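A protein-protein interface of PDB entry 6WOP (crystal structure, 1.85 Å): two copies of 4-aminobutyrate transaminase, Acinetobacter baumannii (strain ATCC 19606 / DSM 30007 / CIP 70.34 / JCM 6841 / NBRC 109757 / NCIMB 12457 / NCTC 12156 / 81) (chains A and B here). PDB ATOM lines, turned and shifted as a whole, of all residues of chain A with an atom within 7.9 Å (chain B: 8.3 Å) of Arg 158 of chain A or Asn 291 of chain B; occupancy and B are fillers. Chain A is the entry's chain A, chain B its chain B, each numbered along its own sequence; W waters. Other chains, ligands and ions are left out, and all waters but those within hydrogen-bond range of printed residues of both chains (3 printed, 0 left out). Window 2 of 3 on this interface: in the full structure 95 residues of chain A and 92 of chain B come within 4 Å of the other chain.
Among the printed residues, pairs that only touch across the chains: Pro 17 of chain A with Met 287 of chain B (3.4 Å), Pro 17 of chain A with Asp 288 of chain B (3.3 Å), Arg 18 of chain A with Pro 292 of chain B (3.4 Å), Gly 19 of chain A with Pro 290 of chain B (3.6 Å), Gly 19 of chain A with Asn 291 of chain B (3.5 Å), Gly 19 of chain A with Pro 292 of chain B (3.7 Å), Val 20 of chain A with Leu 295 of chain B (3.6 Å), Gly 21 of chain A with Gly 293 of chain B (3.8 Å), Arg 142 of chain A with Gly 294 of chain B (3.6 Å), Arg 142 of chain A with Leu 295 of chain B (3.8 Å), Arg 142 of chain A with Gly 296 of chain B (3.6 Å), Pro 155 of chain A with Pro 292 of chain B (3.7 Å), Pro 155 of chain A with Gly 293 of chain B (3.6 Å), Pro 155 of chain A with Gly 294 of chain B (3.7 Å), Arg 158 of chain A with Asn 291 of chain B (3.8 Å), Asp 159 of chain A with Pro 290 of chain B (3.6 Å), Phe 160 of chain A with Pro 290 of chain B (3.997 Å) and Phe 160 of chain A with Gly 294 of chain B (3.2 Å).
Water W2 lies within hydrogen-bond range of O of Leu 295 of chain B, N of Gly 21 of chain A, N of Gly 293 of chain B and O of Gly 19 of chain A.
Water W3 lies within hydrogen-bond range of O of Met 287 of chain B (2.7 Å), N of Gly 19 of chain A (2.7 Å) and O of Pro 290 of chain B (2.9 Å).
Water W1 lies within hydrogen-bond range of the backbone carbonyl oxygen (O) of Asp 288 of chain B (2.8 Å) and the guanidinium group (NH2) of Arg 18 of chain A (3.4 Å).
No position is printed for both chains.
Of the 28 pairs that touch across the chains among the printed residues, none has its exchanged pair printed and touching as well.
The side-chain sulfur (SG) of Cys 125 of chain B is in hydrogen-bond range of the backbone carbonyl oxygen (O) of Ala 289 of chain B (3.8 Å).
The guanidinium group (NE) of Arg 158 of chain A is in salt-bridge range of the side-chain carboxylate (OD1) of Asp 159 of chain A, 3.9 Å away.
The backbone carbonyl oxygen (O) of Thr 153 of chain A sits at hydrogen-bond distance from the backbone NH (N) of Arg 158 of chain A.
Arg 158 of chain A touches one residue of chain B.
Asn 291 of chain B touches four residues of chain A.
Of chain A, only Arg 18, Gly 19 and Pro 155 come within 4 Å of Pro 292 of chain B.
Printed residues of chain A within 4 Å of Pro 290 of chain B: Arg 18, Gly 19, Asp 159 and Phe 160.
Of the printed residues of chain A, Gly 294 of chain B touches Gly 19, Arg 142, Pro 155 and Phe 160.
Tyr 156 of chain A touches none of the printed residues of chain B.
Met 147 of chain A touches none of the printed residues of chain B.
The nearest residue of chain B that does not touch Arg 158 of chain A is Cys 125 of chain B (6.5 Å).
The nearest residue of chain A that does not touch Asn 291 of chain B is Val 20 of chain A (5.3 Å).
Hydrophobic or aromatic side chains of chain B that line the printed part of chain A: Pro 290, Pro 292 and Leu 295.
Along chain B the printed residues that touch a printed residue of chain A span positions 125 to 296.
Hydrophobic or aromatic side chains of chain A that line the printed part of chain B: Pro 17, Pro 155 and Phe 160.
Among the printed residues, 28 pairs touch across the chains.
The backbone carbonyl oxygen of Gly 19 of chain A is in hydrogen-bond range of the backbone NH of Gly 293 of chain B, 3.1 Å away.
O of Gly 19 of chain A sits at hydrogen-bond distance from N of Gly 294 of chain B.
The backbone carbonyl oxygen of Gly 19 of chain A lies within hydrogen-bond range of the backbone NH of Leu 295 of chain B, at 3.1 Å.
NH2 of Arg 18 of chain A lies within hydrogen-bond range of OD1 of Asn 291 of chain B.
NH1 of Arg 142 of chain A is in hydrogen-bond range of O of Gly 293 of chain B (2.8 Å).
OD1 of Asp 159 of chain A is in hydrogen-bond range of ND2 of Asn 291 of chain B, at 2.8 Å.
The backbone carbonyl oxygen (O) of Asp 159 of chain A sits close to the side-chain sulfur (SG) of Cys 125 of chain B (3.6 Å).
NH2 of Arg 18 of chain A lies within hydrogen-bond range of O of Ala 289 of chain B (2.9 Å).
The guanidinium group (NE) of Arg 18 of chain A sits at hydrogen-bond distance from the backbone carbonyl oxygen (O) of Asp 288 of chain B (2.7 Å).
NE of Arg 18 of chain A sits at hydrogen-bond distance from O of Pro 290 of chain B, at 3.4 Å.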
ATOM      1  N   PRO A  17      20.277  23.992   2.653  1.00  0.00           N
ATOM      2  CA  PRO A  17      18.850  24.056   2.332  1.00  0.00           C
ATOM      3  C   PRO A  17      18.462  25.308   1.571  1.00  0.00           C
ATOM      4  O   PRO A  17      19.026  26.384   1.755  1.00  0.00           O
ATOM      5  CB  PRO A  17      18.168  24.031   3.710  1.00  0.00           C
ATOM      6  CG  PRO A  17      19.196  24.291   4.675  1.00  0.00           C
ATOM      7  CD  PRO A  17      20.514  23.962   4.106  1.00  0.00           C
ATOM      8  N   ARG A  18      17.398  25.171   0.787  1.00  0.00           N
ATOM      9  CA  ARG A  18      16.878  26.335   0.091  1.00  0.00           C
ATOM     10  C   ARG A  18      16.268  27.356   1.034  1.00  0.00           C
ATOM     11  O   ARG A  18      16.048  28.505   0.612  1.00  0.00           O
ATOM     12  CB  ARG A  18      15.851  25.911  -0.950  1.00  0.00           C
ATOM     13  CG  ARG A  18      14.514  25.640  -0.356  1.00  0.00           C
ATOM     14  CD  ARG A  18      13.592  24.965  -1.382  1.00  0.00           C
ATOM     15  NE  ARG A  18      12.444  24.490  -0.622  1.00  0.00           N
ATOM     16  CZ  ARG A  18      11.213  24.905  -0.781  1.00  0.00           C
ATOM     17  NH1 ARG A  18      10.914  25.774  -1.756  1.00  0.00           N
ATOM     18  NH2 ARG A  18      10.254  24.392   0.002  1.00  0.00           N
ATOM     19  N   GLY A  19      16.008  26.979   2.289  1.00  0.00           N
ATOM     20  CA  GLY A  19      15.276  27.857   3.202  1.00  0.00           C
ATOM     21  C   GLY A  19      16.073  29.073   3.605  1.00  0.00           C
ATOM     22  O   GLY A  19      15.507  30.117   3.903  1.00  0.00           O
ATOM     23  N   VAL A  20      17.388  28.986   3.542  1.00  0.00           N
ATOM     24  CA  VAL A  20      18.198  30.192   3.710  1.00  0.00           C
ATOM     25  C   VAL A  20      18.234  30.954   2.388  1.00  0.00           C
ATOM     26  O   VAL A  20      18.937  30.539   1.474  1.00  0.00           O
ATOM     27  CB  VAL A  20      19.616  29.844   4.169  1.00  0.00           C
ATOM     28  CG1 VAL A  20      20.304  31.151   4.651  1.00  0.00           C
ATOM     29  CG2 VAL A  20      19.561  28.769   5.253  1.00  0.00           C
ATOM     30  N   GLY A  21      17.521  32.081   2.308  1.00  0.00           N
ATOM     31  CA  GLY A  21      17.512  32.881   1.085  1.00  0.00           C
ATOM     32  C   GLY A  21      18.759  33.775   1.017  1.00  0.00           C
ATOM     33  O   GLY A  21      19.082  34.494   1.974  1.00  0.00           O
ATOM     34  N   ARG A 142      13.485  35.187  14.870  1.00  0.00           N
ATOM     35  CA  ARG A 142      13.021  34.010  14.168  1.00  0.00           C
ATOM     36  C   ARG A 142      12.784  32.821  15.097  1.00  0.00           C
ATOM     37  O   ARG A 142      12.646  31.698  14.614  1.00  0.00           O
ATOM     38  CB  ARG A 142      14.049  33.664  13.090  1.00  0.00           C
ATOM     39  CG  ARG A 142      14.090  34.674  11.956  1.00  0.00           C
ATOM     40  CD  ARG A 142      15.207  34.193  10.938  1.00  0.00           C
ATOM     41  NE  ARG A 142      15.319  35.054   9.754  1.00  0.00           N
ATOM     42  CZ  ARG A 142      14.626  34.824   8.635  1.00  0.00           C
ATOM     43  NH1 ARG A 142      13.733  33.792   8.584  1.00  0.00           N
ATOM     44  NH2 ARG A 142      14.823  35.619   7.572  1.00  0.00           N
ATOM     45  N   MET A 147       9.006  35.053  16.388  1.00  0.00           N
ATOM     46  CA  MET A 147       8.243  35.013  15.138  1.00  0.00           C
ATOM     47  C   MET A 147       6.802  35.438  15.383  1.00  0.00           C
ATOM     48  O   MET A 147       6.194  36.098  14.535  1.00  0.00           O
ATOM     49  CB  MET A 147       8.203  33.575  14.550  1.00  0.00           C
ATOM     50  CG  MET A 147       9.386  33.229  13.759  1.00  0.00           C
ATOM     51  SD  MET A 147       9.016  31.573  12.959  1.00  0.00           S
ATOM     52  CE  MET A 147       9.280  30.403  14.276  1.00  0.00           C
ATOM     53  N   LYS A 152       4.819  40.071  10.408  1.00  0.00           N
ATOM     54  CA  LYS A 152       4.867  39.750   9.010  1.00  0.00           C
ATOM     55  C   LYS A 152       4.886  38.236   8.901  1.00  0.00           C
ATOM     56  O   LYS A 152       5.788  37.621   9.322  1.00  0.00           O
ATOM     57  CB  LYS A 152       6.083  40.416   8.369  1.00  0.00           C
ATOM     58  CG  LYS A 152       6.198  40.232   6.880  1.00  0.00           C
ATOM     59  CD  LYS A 152       7.150  41.217   6.240  1.00  0.00           C
ATOM     60  CE  LYS A 152       7.551  40.823   4.823  1.00  0.00           C
ATOM     61  NZ  LYS A 152       8.421  41.870   4.230  1.00  0.00           N
ATOM     62  N   THR A 153       3.915  37.655   8.250  1.00  0.00           N
ATOM     63  CA  THR A 153       3.867  36.206   8.251  1.00  0.00           C
ATOM     64  C   THR A 153       4.717  35.653   7.128  1.00  0.00           C
ATOM     65  O   THR A 153       5.287  34.565   7.264  1.00  0.00           O
ATOM     66  CB  THR A 153       2.415  35.747   8.091  1.00  0.00           C
ATOM     67  OG1 THR A 153       1.891  36.316   6.902  1.00  0.00           O
ATOM     68  CG2 THR A 153       1.604  36.296   9.205  1.00  0.00           C
ATOM     69  N   ALA A 154       4.798  36.370   5.988  1.00  0.00           N
ATOM     70  CA  ALA A 154       5.570  35.769   4.900  1.00  0.00           C
ATOM     71  C   ALA A 154       6.818  36.584   4.683  1.00  0.00           C
ATOM     72  O   ALA A 154       6.691  37.802   4.559  1.00  0.00           O
ATOM     73  CB  ALA A 154       4.743  35.748   3.622  1.00  0.00           C
ATOM     74  N   PRO A 155       8.027  35.975   4.583  1.00  0.00           N
ATOM     75  CA  PRO A 155       8.331  34.538   4.568  1.00  0.00           C
ATOM     76  C   PRO A 155       8.584  33.923   5.954  1.00  0.00           C
ATOM     77  O   PRO A 155       8.839  32.724   6.011  1.00  0.00           O
ATOM     78  CB  PRO A 155       9.658  34.484   3.768  1.00  0.00           C
ATOM     79  CG  PRO A 155      10.371  35.696   4.285  1.00  0.00           C
ATOM     80  CD  PRO A 155       9.265  36.783   4.482  1.00  0.00           C
ATOM     81  N   TYR A 156       8.505  34.730   7.023  1.00  0.00           N
ATOM     82  CA  TYR A 156       9.154  34.389   8.285  1.00  0.00           C
ATOM     83  C   TYR A 156       8.434  33.278   9.033  1.00  0.00           C
ATOM     84  O   TYR A 156       9.077  32.442   9.678  1.00  0.00           O
ATOM     85  CB  TYR A 156       9.229  35.615   9.220  1.00  0.00           C
ATOM     86  CG  TYR A 156       9.980  36.742   8.576  1.00  0.00           C
ATOM     87  CD1 TYR A 156      11.284  36.559   8.118  1.00  0.00           C
ATOM     88  CD2 TYR A 156       9.391  37.981   8.398  1.00  0.00           C
ATOM     89  CE1 TYR A 156      11.972  37.591   7.494  1.00  0.00           C
ATOM     90  CE2 TYR A 156      10.063  39.004   7.794  1.00  0.00           C
ATOM     91  CZ  TYR A 156      11.354  38.810   7.333  1.00  0.00           C
ATOM     92  OH  TYR A 156      12.004  39.843   6.709  1.00  0.00           O
ATOM     93  N   LYS A 157       7.122  33.274   9.043  1.00  0.00           N
ATOM     94  CA  LYS A 157       6.499  32.261   9.905  1.00  0.00           C
ATOM     95  C   LYS A 157       5.426  31.422   9.242  1.00  0.00           C
ATOM     96  O   LYS A 157       4.975  30.467   9.881  1.00  0.00           O
ATOM     97  CB  LYS A 157       5.936  32.902  11.192  1.00  0.00           C
ATOM     98  CG  LYS A 157       4.887  33.910  10.980  1.00  0.00           C
ATOM     99  CD  LYS A 157       4.582  34.641  12.342  1.00  0.00           C
ATOM    100  CE  LYS A 157       3.649  35.792  12.231  1.00  0.00           C
ATOM    101  NZ  LYS A 157       3.509  36.643  13.481  1.00  0.00           N
ATOM    102  N   ARG A 158       5.076  31.679   7.951  1.00  0.00           N
ATOM    103  CA  ARG A 158       4.064  30.888   7.245  1.00  0.00           C
ATOM    104  C   ARG A 158       4.375  29.379   7.181  1.00  0.00           C
ATOM    105  O   ARG A 158       3.465  28.565   6.945  1.00  0.00           O
ATOM    106  CB  ARG A 158       3.897  31.441   5.825  1.00  0.00           C
ATOM    107  CG  ARG A 158       5.180  31.329   4.995  1.00  0.00           C
ATOM    108  CD  ARG A 158       4.931  31.099   3.516  1.00  0.00           C
ATOM    109  NE  ARG A 158       3.953  30.040   3.297  1.00  0.00           N
ATOM    110  CZ  ARG A 158       3.767  29.400   2.139  1.00  0.00           C
ATOM    111  NH1 ARG A 158       4.518  29.708   1.086  1.00  0.00           N
ATOM    112  NH2 ARG A 158       2.823  28.456   2.022  1.00  0.00           N
ATOM    113  N   ASP A 159       5.640  28.980   7.273  1.00  0.00           N
ATOM    114  CA  ASP A 159       5.959  27.561   7.138  1.00  0.00           C
ATOM    115  C   ASP A 159       5.806  26.801   8.453  1.00  0.00           C
ATOM    116  O   ASP A 159       5.974  25.583   8.449  1.00  0.00           O
ATOM    117  CB  ASP A 159       7.437  27.382   6.685  1.00  0.00           C
ATOM    118  CG  ASP A 159       7.677  27.747   5.247  1.00  0.00           C
ATOM    119  OD1 ASP A 159       6.751  27.620   4.447  1.00  0.00           O
ATOM    120  OD2 ASP A 159       8.814  28.196   4.951  1.00  0.00           O
ATOM    121  N   PHE A 160       5.609  27.482   9.594  1.00  0.00           N
ATOM    122  CA  PHE A 160       5.927  26.850  10.883  1.00  0.00           C
ATOM    123  C   PHE A 160       4.724  26.702  11.827  1.00  0.00           C
ATOM    124  O   PHE A 160       4.909  26.321  12.997  1.00  0.00           O
ATOM    125  CB  PHE A 160       7.080  27.585  11.593  1.00  0.00           C
ATOM    126  CG  PHE A 160       8.300  27.742  10.705  1.00  0.00           C
ATOM    127  CD1 PHE A 160       8.887  26.633  10.136  1.00  0.00           C
ATOM    128  CD2 PHE A 160       8.778  29.005  10.378  1.00  0.00           C
ATOM    129  CE1 PHE A 160      10.012  26.778   9.254  1.00  0.00           C
ATOM    130  CE2 PHE A 160       9.861  29.172   9.527  1.00  0.00           C
ATOM    131  CZ  PHE A 160      10.484  28.065   8.971  1.00  0.00           C
ATOM    132  N   GLY A 161       3.497  26.792  11.314  1.00  0.00           N
ATOM    133  CA  GLY A 161       2.379  26.276  12.133  1.00  0.00           C
ATOM    134  C   GLY A 161       2.024  27.177  13.309  1.00  0.00           C
ATOM    135  O   GLY A 161       2.214  28.397  13.292  1.00  0.00           O
ATOM    136  N   MET A 163       1.483  29.389  16.589  1.00  0.00           N
ATOM    137  CA  MET A 163       2.397  30.312  17.268  1.00  0.00           C
ATOM    138  C   MET A 163       1.951  30.369  18.723  1.00  0.00           C
ATOM    139  O   MET A 163       0.777  30.108  19.015  1.00  0.00           O
ATOM    140  CB  MET A 163       2.348  31.734  16.677  1.00  0.00           C
ATOM    141  CG  MET A 163       2.864  31.843  15.224  1.00  0.00           C
ATOM    142  SD  MET A 163       4.683  31.628  15.368  1.00  0.00           S
ATOM    143  CE  MET A 163       5.035  30.265  14.228  1.00  0.00           C
ATOM    144  N   CYS B 125       7.672  22.000   9.562  1.00  0.00           N
ATOM    145  CA  CYS B 125       7.265  22.343   8.204  1.00  0.00           C
ATOM    146  C   CYS B 125       7.304  21.116   7.312  1.00  0.00           C
ATOM    147  O   CYS B 125       6.340  20.847   6.573  1.00  0.00           O
ATOM    148  CB  CYS B 125       8.153  23.457   7.641  1.00  0.00           C
ATOM    149  SG  CYS B 125       7.771  23.834   5.891  1.00  0.00           S
ATOM    150  N   MET B 287      15.478  18.994   5.292  1.00  0.00           N
ATOM    151  CA  MET B 287      16.081  20.333   5.405  1.00  0.00           C
ATOM    152  C   MET B 287      15.491  21.281   4.361  1.00  0.00           C
ATOM    153  O   MET B 287      15.316  22.477   4.629  1.00  0.00           O
ATOM    154  CB  MET B 287      17.601  20.248   5.192  1.00  0.00           C
ATOM    155  CG  MET B 287      18.343  19.380   6.227  1.00  0.00           C
ATOM    156  SD  MET B 287      18.317  20.142   7.908  1.00  0.00           S
ATOM    157  CE  MET B 287      19.401  21.585   7.625  1.00  0.00           C
ATOM    158  N   ASP B 288      15.119  20.742   3.198  1.00  0.00           N
ATOM    159  CA  ASP B 288      14.646  21.571   2.105  1.00  0.00           C
ATOM    160  C   ASP B 288      13.173  21.956   2.263  1.00  0.00           C
ATOM    161  O   ASP B 288      12.632  22.636   1.385  1.00  0.00           O
ATOM    162  CB  ASP B 288      14.864  20.854   0.769  1.00  0.00           C
ATOM    163  CG  ASP B 288      16.223  21.176   0.175  1.00  0.00           C
ATOM    164  OD1 ASP B 288      16.807  22.248   0.508  1.00  0.00           O
ATOM    165  OD2 ASP B 288      16.705  20.363  -0.622  1.00  0.00           O
ATOM    166  N   ALA B 289      12.534  21.557   3.352  1.00  0.00           N
ATOM    167  CA  ALA B 289      11.097  21.790   3.458  1.00  0.00           C
ATOM    168  C   ALA B 289      10.775  23.277   3.573  1.00  0.00           C
ATOM    169  O   ALA B 289       9.914  23.749   2.814  1.00  0.00           O
ATOM    170  CB  ALA B 289      10.514  20.966   4.617  1.00  0.00           C
ATOM    171  N   PRO B 290      11.399  24.061   4.463  1.00  0.00           N
ATOM    172  CA  PRO B 290      11.084  25.490   4.515  1.00  0.00           C
ATOM    173  C   PRO B 290      11.378  26.190   3.198  1.00  0.00           C
ATOM    174  O   PRO B 290      12.332  25.857   2.477  1.00  0.00           O
ATOM    175  CB  PRO B 290      12.003  26.011   5.634  1.00  0.00           C
ATOM    176  CG  PRO B 290      12.202  24.849   6.523  1.00  0.00           C
ATOM    177  CD  PRO B 290      12.306  23.680   5.566  1.00  0.00           C
ATOM    178  N   ASN B 291      10.553  27.206   2.906  1.00  0.00           N
ATOM    179  CA  ASN B 291      10.710  28.007   1.702  1.00  0.00           C
ATOM    180  C   ASN B 291      11.796  29.073   1.885  1.00  0.00           C
ATOM    181  O   ASN B 291      12.117  29.451   3.010  1.00  0.00           O
ATOM    182  CB  ASN B 291       9.362  28.630   1.345  1.00  0.00           C
ATOM    183  CG  ASN B 291       8.367  27.564   0.893  1.00  0.00           C
ATOM    184  OD1 ASN B 291       8.595  26.926  -0.153  1.00  0.00           O
ATOM    185  ND2 ASN B 291       7.341  27.275   1.717  1.00  0.00           N
ATOM    186  N   PRO B 292      12.369  29.587   0.783  1.00  0.00           N
ATOM    187  CA  PRO B 292      13.393  30.660   0.912  1.00  0.00           C
ATOM    188  C   PRO B 292      12.877  31.817   1.758  1.00  0.00           C
ATOM    189  O   PRO B 292      11.735  32.257   1.608  1.00  0.00           O
ATOM    190  CB  PRO B 292      13.639  31.114  -0.549  1.00  0.00           C
ATOM    191  CG  PRO B 292      13.341  29.886  -1.375  1.00  0.00           C
ATOM    192  CD  PRO B 292      12.155  29.187  -0.628  1.00  0.00           C
ATOM    193  N   GLY B 293      13.735  32.297   2.662  1.00  0.00           N
ATOM    194  CA  GLY B 293      13.429  33.314   3.635  1.00  0.00           C
ATOM    195  C   GLY B 293      12.908  32.755   4.938  1.00  0.00           C
ATOM    196  O   GLY B 293      12.777  33.515   5.924  1.00  0.00           O
ATOM    197  N   GLY B 294      12.549  31.470   4.939  1.00  0.00           N
ATOM    198  CA  GLY B 294      12.022  30.767   6.105  1.00  0.00           C
ATOM    199  C   GLY B 294      13.059  30.482   7.176  1.00  0.00           C
ATOM    200  O   GLY B 294      12.689  30.313   8.337  1.00  0.00           O
ATOM    201  N   LEU B 295      14.356  30.435   6.816  1.00  0.00           N
ATOM    202  CA  LEU B 295      15.450  30.225   7.751  1.00  0.00           C
ATOM    203  C   LEU B 295      16.499  31.327   7.591  1.00  0.00           C
ATOM    204  O   LEU B 295      16.710  31.865   6.503  1.00  0.00           O
ATOM    205  CB  LEU B 295      16.169  28.902   7.495  1.00  0.00           C
ATOM    206  CG  LEU B 295      15.196  27.736   7.474  1.00  0.00           C
ATOM    207  CD1 LEU B 295      16.008  26.503   6.858  1.00  0.00           C
ATOM    208  CD2 LEU B 295      14.724  27.447   8.909  1.00  0.00           C
ATOM    209  N   GLY B 296      17.129  31.664   8.675  1.00  0.00           N
ATOM    210  CA  GLY B 296      18.294  32.556   8.550  1.00  0.00           C
ATOM    211  C   GLY B 296      18.623  33.164   9.906  1.00  0.00           C
ATOM    212  O   GLY B 296      18.365  32.561  10.963  1.00  0.00           O
HETATM  213  O   HOH W   1      11.146  21.190  -0.483  1.00  0.00           O
HETATM  214  O   HOH W   2      16.524  33.415   4.418  1.00  0.00           O
HETATM  215  O   HOH W   3      14.829  24.827   3.478  1.00  0.00           O
